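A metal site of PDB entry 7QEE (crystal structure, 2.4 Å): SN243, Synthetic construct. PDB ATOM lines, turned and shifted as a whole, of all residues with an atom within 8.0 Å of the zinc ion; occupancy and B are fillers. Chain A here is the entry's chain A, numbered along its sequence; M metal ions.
The side-chain amide oxygen (OD1) of Asn 35 is in hydrogen-bond range of the backbone NH (N) of Glu 37 (3.0 Å).
The side-chain amide oxygen (OD1) of Asn 33 sits close to the side-chain carboxylate (OD1) of Asp 31, at 2.8 Å.
The side-chain hydroxyl (OH) of Tyr 41 lies within hydrogen-bond range of the backbone NH (N) of Asn 33 (3.4 Å).
The side-chain amide oxygen (OD1) of Asn 35 sits close to the side-chain carboxylate (OD1) of Asp 31.
ND2 of Asn 35 sits at hydrogen-bond distance from OD1 of Asp 39, at 3.0 Å.
The side-chain carboxylate of Asp 31 sits at hydrogen-bond distance from the backbone NH of Gly 36 (3.1 Å).
The backbone NH (N) of Asp 31 lies within hydrogen-bond range of the backbone carbonyl oxygen (O) of Glu 20, 2.8 Å away.
The side-chain carboxylate (OD2) of Asp 39 lies within hydrogen-bond range of the side-chain amide nitrogen (NE2) of Gln 58 (3.1 Å).
The zinc ion is bound by O of Glu 37 (2.1 Å), OE1 of Glu 42 (2.2 Å) and OD1 of Asn 33 (2.5 Å).
Slightly farther from the zinc ion lies the side-chain carboxylate (OE2) of Glu 42 (2.6 Å).
Slightly farther from the zinc ion lies OD1 of Asn 35 (2.7 Å).
Slightly farther from the zinc ion lies OD1 of Asp 31 (2.7 Å).
Slightly farther from the zinc ion lies OD1 of Asp 39 (2.8 Å).
CA of Leu 38 touches the zinc ion, at 3.9 Å.
Within 4 Å of the zinc ion: Asp 31, Asn 33, Asn 35, Glu 37, Leu 38, Asp 39 and Glu 42.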
ATOM      1  N   GLU A  20     -20.072   4.503 -31.917  1.00  0.00           N
ATOM      2  CA  GLU A  20     -20.575   3.233 -32.409  1.00  0.00           C
ATOM      3  C   GLU A  20     -20.330   2.128 -31.389  1.00  0.00           C
ATOM      4  O   GLU A  20     -19.396   2.200 -30.595  1.00  0.00           O
ATOM      5  CB  GLU A  20     -19.901   2.860 -33.744  1.00  0.00           C
ATOM      6  CG  GLU A  20     -20.670   3.248 -35.023  1.00  0.00           C
ATOM      7  CD  GLU A  20     -20.157   4.543 -35.672  1.00  0.00           C
ATOM      8  OE1 GLU A  20     -19.127   5.091 -35.213  1.00  0.00           O
ATOM      9  OE2 GLU A  20     -20.775   5.000 -36.654  1.00  0.00           O
ATOM     10  N   ILE A  22     -19.422  -1.967 -30.662  1.00  0.00           N
ATOM     11  CA  ILE A  22     -18.625  -2.960 -31.352  1.00  0.00           C
ATOM     12  C   ILE A  22     -18.681  -4.276 -30.591  1.00  0.00           C
ATOM     13  O   ILE A  22     -18.664  -4.307 -29.349  1.00  0.00           O
ATOM     14  CB  ILE A  22     -17.154  -2.568 -31.583  1.00  0.00           C
ATOM     15  CG1 ILE A  22     -16.383  -2.496 -30.261  1.00  0.00           C
ATOM     16  CG2 ILE A  22     -17.075  -1.327 -32.446  1.00  0.00           C
ATOM     17  CD1 ILE A  22     -15.019  -1.844 -30.377  1.00  0.00           C
ATOM     18  N   PHE A  29     -19.657  -3.567 -26.598  1.00  0.00           N
ATOM     19  CA  PHE A  29     -18.811  -2.533 -26.018  1.00  0.00           C
ATOM     20  C   PHE A  29     -18.996  -1.250 -26.815  1.00  0.00           C
ATOM     21  O   PHE A  29     -19.307  -1.295 -28.004  1.00  0.00           O
ATOM     22  CB  PHE A  29     -17.319  -2.932 -26.048  1.00  0.00           C
ATOM     23  CG  PHE A  29     -17.018  -4.257 -25.374  1.00  0.00           C
ATOM     24  CD1 PHE A  29     -16.768  -4.320 -24.002  1.00  0.00           C
ATOM     25  CD2 PHE A  29     -16.974  -5.429 -26.106  1.00  0.00           C
ATOM     26  CE1 PHE A  29     -16.493  -5.537 -23.381  1.00  0.00           C
ATOM     27  CE2 PHE A  29     -16.691  -6.649 -25.490  1.00  0.00           C
ATOM     28  CZ  PHE A  29     -16.445  -6.710 -24.126  1.00  0.00           C
ATOM     29  N   ARG A  30     -18.770  -0.110 -26.163  1.00  0.00           N
ATOM     30  CA  ARG A  30     -18.843   1.191 -26.831  1.00  0.00           C
ATOM     31  C   ARG A  30     -17.471   1.642 -27.320  1.00  0.00           C
ATOM     32  O   ARG A  30     -16.519   1.688 -26.543  1.00  0.00           O
ATOM     33  CB  ARG A  30     -19.424   2.256 -25.915  1.00  0.00           C
ATOM     34  CG  ARG A  30     -20.886   2.048 -25.620  1.00  0.00           C
ATOM     35  CD  ARG A  30     -21.354   2.879 -24.439  1.00  0.00           C
ATOM     36  NE  ARG A  30     -21.722   4.249 -24.816  1.00  0.00           N
ATOM     37  CZ  ARG A  30     -21.512   5.303 -24.035  1.00  0.00           C
ATOM     38  NH1 ARG A  30     -21.876   6.515 -24.430  1.00  0.00           N
ATOM     39  NH2 ARG A  30     -20.940   5.123 -22.851  1.00  0.00           N
ATOM     40  N   ASP A  31     -17.391   2.011 -28.603  1.00  0.00           N
ATOM     41  CA  ASP A  31     -16.134   2.435 -29.222  1.00  0.00           C
ATOM     42  C   ASP A  31     -15.959   3.949 -29.047  1.00  0.00           C
ATOM     43  O   ASP A  31     -16.109   4.753 -29.973  1.00  0.00           O
ATOM     44  CB  ASP A  31     -16.117   2.046 -30.695  1.00  0.00           C
ATOM     45  CG  ASP A  31     -14.914   2.600 -31.439  1.00  0.00           C
ATOM     46  OD1 ASP A  31     -13.803   2.493 -30.897  1.00  0.00           O
ATOM     47  OD2 ASP A  31     -15.085   3.139 -32.561  1.00  0.00           O
ATOM     48  N   LEU A  32     -15.615   4.327 -27.806  1.00  0.00           N
ATOM     49  CA  LEU A  32     -15.709   5.726 -27.389  1.00  0.00           C
ATOM     50  C   LEU A  32     -14.633   6.610 -28.002  1.00  0.00           C
ATOM     51  O   LEU A  32     -14.784   7.834 -28.033  1.00  0.00           O
ATOM     52  CB  LEU A  32     -15.671   5.808 -25.860  1.00  0.00           C
ATOM     53  CG  LEU A  32     -16.966   5.422 -25.127  1.00  0.00           C
ATOM     54  CD1 LEU A  32     -16.665   5.106 -23.694  1.00  0.00           C
ATOM     55  CD2 LEU A  32     -17.974   6.564 -25.198  1.00  0.00           C
ATOM     56  N   ASN A  33     -13.506   6.030 -28.423  1.00  0.00           N
ATOM     57  CA  ASN A  33     -12.456   6.768 -29.105  1.00  0.00           C
ATOM     58  C   ASN A  33     -12.611   6.756 -30.621  1.00  0.00           C
ATOM     59  O   ASN A  33     -11.762   7.329 -31.312  1.00  0.00           O
ATOM     60  CB  ASN A  33     -11.095   6.197 -28.726  1.00  0.00           C
ATOM     61  CG  ASN A  33     -10.958   4.729 -29.102  1.00  0.00           C
ATOM     62  OD1 ASN A  33     -11.814   4.159 -29.795  1.00  0.00           O
ATOM     63  ND2 ASN A  33      -9.890   4.101 -28.619  1.00  0.00           N
ATOM     64  N   ASP A  34     -13.642   6.065 -31.150  1.00  0.00           N
ATOM     65  CA  ASP A  34     -13.953   6.046 -32.579  1.00  0.00           C
ATOM     66  C   ASP A  34     -12.794   5.458 -33.385  1.00  0.00           C
ATOM     67  O   ASP A  34     -12.545   5.868 -34.519  1.00  0.00           O
ATOM     68  CB  ASP A  34     -14.335   7.422 -33.135  1.00  0.00           C
ATOM     69  CG  ASP A  34     -15.240   7.326 -34.387  1.00  0.00           C
ATOM     70  OD1 ASP A  34     -15.841   6.241 -34.601  1.00  0.00           O
ATOM     71  OD2 ASP A  34     -15.335   8.313 -35.157  1.00  0.00           O
ATOM     72  N   ASN A  35     -12.023   4.561 -32.765  1.00  0.00           N
ATOM     73  CA  ASN A  35     -10.896   3.945 -33.455  1.00  0.00           C
ATOM     74  C   ASN A  35     -11.227   2.570 -34.012  1.00  0.00           C
ATOM     75  O   ASN A  35     -10.318   1.898 -34.520  1.00  0.00           O
ATOM     76  CB  ASN A  35      -9.677   3.884 -32.538  1.00  0.00           C
ATOM     77  CG  ASN A  35      -9.769   2.784 -31.513  1.00  0.00           C
ATOM     78  OD1 ASN A  35     -10.796   2.155 -31.359  1.00  0.00           O
ATOM     79  ND2 ASN A  35      -8.666   2.522 -30.817  1.00  0.00           N
ATOM     80  N   GLY A  36     -12.453   2.103 -33.880  1.00  0.00           N
ATOM     81  CA  GLY A  36     -12.844   0.845 -34.469  1.00  0.00           C
ATOM     82  C   GLY A  36     -12.415  -0.399 -33.729  1.00  0.00           C
ATOM     83  O   GLY A  36     -12.971  -1.476 -33.990  1.00  0.00           O
ATOM     84  N   GLU A  37     -11.425  -0.308 -32.856  1.00  0.00           N
ATOM     85  CA  GLU A  37     -11.060  -1.442 -32.018  1.00  0.00           C
ATOM     86  C   GLU A  37     -11.350  -1.131 -30.552  1.00  0.00           C
ATOM     87  O   GLU A  37     -11.567   0.014 -30.153  1.00  0.00           O
ATOM     88  CB  GLU A  37      -9.604  -1.848 -32.253  1.00  0.00           C
ATOM     89  CG  GLU A  37      -9.277  -1.980 -33.743  1.00  0.00           C
ATOM     90  CD  GLU A  37      -9.277  -3.426 -34.247  1.00  0.00           C
ATOM     91  OE1 GLU A  37      -9.224  -3.631 -35.483  1.00  0.00           O
ATOM     92  OE2 GLU A  37      -9.362  -4.358 -33.421  1.00  0.00           O
ATOM     93  N   LEU A  38     -11.357  -2.173 -29.726  1.00  0.00           N
ATOM     94  CA  LEU A  38     -11.758  -2.053 -28.326  1.00  0.00           C
ATOM     95  C   LEU A  38     -10.547  -1.782 -27.439  1.00  0.00           C
ATOM     96  O   LEU A  38      -9.700  -2.666 -27.260  1.00  0.00           O
ATOM     97  CB  LEU A  38     -12.492  -3.324 -27.899  1.00  0.00           C
ATOM     98  CG  LEU A  38     -12.689  -3.521 -26.400  1.00  0.00           C
ATOM     99  CD1 LEU A  38     -13.797  -2.613 -25.908  1.00  0.00           C
ATOM    100  CD2 LEU A  38     -13.008  -4.965 -26.087  1.00  0.00           C
ATOM    101  N   ASP A  39     -10.454  -0.560 -26.879  1.00  0.00           N
ATOM    102  CA  ASP A  39      -9.441  -0.220 -25.874  1.00  0.00           C
ATOM    103  C   ASP A  39      -9.778  -0.806 -24.511  1.00  0.00           C
ATOM    104  O   ASP A  39     -10.943  -1.103 -24.207  1.00  0.00           O
ATOM    105  CB  ASP A  39      -9.283   1.281 -25.740  1.00  0.00           C
ATOM    106  CG  ASP A  39      -8.832   1.928 -27.011  1.00  0.00           C
ATOM    107  OD1 ASP A  39      -9.320   1.524 -28.083  1.00  0.00           O
ATOM    108  OD2 ASP A  39      -8.002   2.862 -26.942  1.00  0.00           O
ATOM    109  N   PRO A  40      -8.767  -0.995 -23.650  1.00  0.00           N
ATOM    110  CA  PRO A  40      -9.057  -1.428 -22.264  1.00  0.00           C
ATOM    111  C   PRO A  40     -10.045  -0.545 -21.517  1.00  0.00           C
ATOM    112  O   PRO A  40     -10.858  -1.062 -20.737  1.00  0.00           O
ATOM    113  CB  PRO A  40      -7.674  -1.401 -21.607  1.00  0.00           C
ATOM    114  CG  PRO A  40      -6.722  -1.637 -22.724  1.00  0.00           C
ATOM    115  CD  PRO A  40      -7.323  -0.961 -23.932  1.00  0.00           C
ATOM    116  N   TYR A  41      -9.999   0.783 -21.727  1.00  0.00           N
ATOM    117  CA  TYR A  41     -10.892   1.667 -20.986  1.00  0.00           C
ATOM    118  C   TYR A  41     -12.345   1.545 -21.439  1.00  0.00           C
ATOM    119  O   TYR A  41     -13.254   1.885 -20.684  1.00  0.00           O
ATOM    120  CB  TYR A  41     -10.395   3.111 -21.059  1.00  0.00           C
ATOM    121  CG  TYR A  41     -10.878   3.955 -22.197  1.00  0.00           C
ATOM    122  CD1 TYR A  41     -12.029   4.720 -22.069  1.00  0.00           C
ATOM    123  CD2 TYR A  41     -10.155   4.062 -23.369  1.00  0.00           C
ATOM    124  CE1 TYR A  41     -12.478   5.536 -23.104  1.00  0.00           C
ATOM    125  CE2 TYR A  41     -10.601   4.878 -24.418  1.00  0.00           C
ATOM    126  CZ  TYR A  41     -11.760   5.612 -24.270  1.00  0.00           C
ATOM    127  OH  TYR A  41     -12.213   6.428 -25.291  1.00  0.00           O
ATOM    128  N   GLU A  42     -12.573   1.085 -22.673  1.00  0.00           N
ATOM    129  CA  GLU A  42     -13.903   0.766 -23.151  1.00  0.00           C
ATOM    130  C   GLU A  42     -14.340  -0.654 -22.765  1.00  0.00           C
ATOM    131  O   GLU A  42     -15.488  -1.037 -23.045  1.00  0.00           O
ATOM    132  CB  GLU A  42     -13.955   0.941 -24.667  1.00  0.00           C
ATOM    133  CG  GLU A  42     -13.550   2.345 -25.133  1.00  0.00           C
ATOM    134  CD  GLU A  42     -12.982   2.339 -26.552  1.00  0.00           C
ATOM    135  OE1 GLU A  42     -12.457   1.272 -26.965  1.00  0.00           O
ATOM    136  OE2 GLU A  42     -13.053   3.388 -27.237  1.00  0.00           O
ATOM    137  N   ASP A  43     -13.469  -1.437 -22.138  1.00  0.00           N
ATOM    138  CA  ASP A  43     -13.716  -2.850 -21.859  1.00  0.00           C
ATOM    139  C   ASP A  43     -14.257  -2.991 -20.445  1.00  0.00           C
ATOM    140  O   ASP A  43     -13.505  -3.121 -19.480  1.00  0.00           O
ATOM    141  CB  ASP A  43     -12.426  -3.646 -22.061  1.00  0.00           C
ATOM    142  CG  ASP A  43     -12.630  -5.140 -21.908  1.00  0.00           C
ATOM    143  OD1 ASP A  43     -13.420  -5.565 -21.037  1.00  0.00           O
ATOM    144  OD2 ASP A  43     -12.011  -5.900 -22.675  1.00  0.00           O
ATOM    145  N   ASP A  54      -5.534   2.939 -18.648  1.00  0.00           N
ATOM    146  CA  ASP A  54      -5.532   2.977 -20.111  1.00  0.00           C
ATOM    147  C   ASP A  54      -6.096   4.295 -20.637  1.00  0.00           C
ATOM    148  O   ASP A  54      -5.701   4.759 -21.722  1.00  0.00           O
ATOM    149  CB  ASP A  54      -6.297   1.800 -20.690  1.00  0.00           C
ATOM    150  CG  ASP A  54      -6.215   1.762 -22.206  1.00  0.00           C
ATOM    151  OD1 ASP A  54      -5.271   1.165 -22.751  1.00  0.00           O
ATOM    152  OD2 ASP A  54      -7.078   2.374 -22.857  1.00  0.00           O
ATOM    153  N   GLN A  58      -4.058   7.942 -22.785  1.00  0.00           N
ATOM    154  CA  GLN A  58      -4.409   8.499 -24.082  1.00  0.00           C
ATOM    155  C   GLN A  58      -4.844   9.960 -24.034  1.00  0.00           C
ATOM    156  O   GLN A  58      -5.346  10.464 -25.046  1.00  0.00           O
ATOM    157  CB  GLN A  58      -5.534   7.676 -24.698  1.00  0.00           C
ATOM    158  CG  GLN A  58      -5.350   6.193 -24.574  1.00  0.00           C
ATOM    159  CD  GLN A  58      -6.552   5.444 -25.116  1.00  0.00           C
ATOM    160  OE1 GLN A  58      -7.180   5.882 -26.085  1.00  0.00           O
ATOM    161  NE2 GLN A  58      -6.862   4.305 -24.507  1.00  0.00           N
HETATM  162 ZN    ZN M   1     -11.968   1.765 -29.002  1.00  0.00          ZN
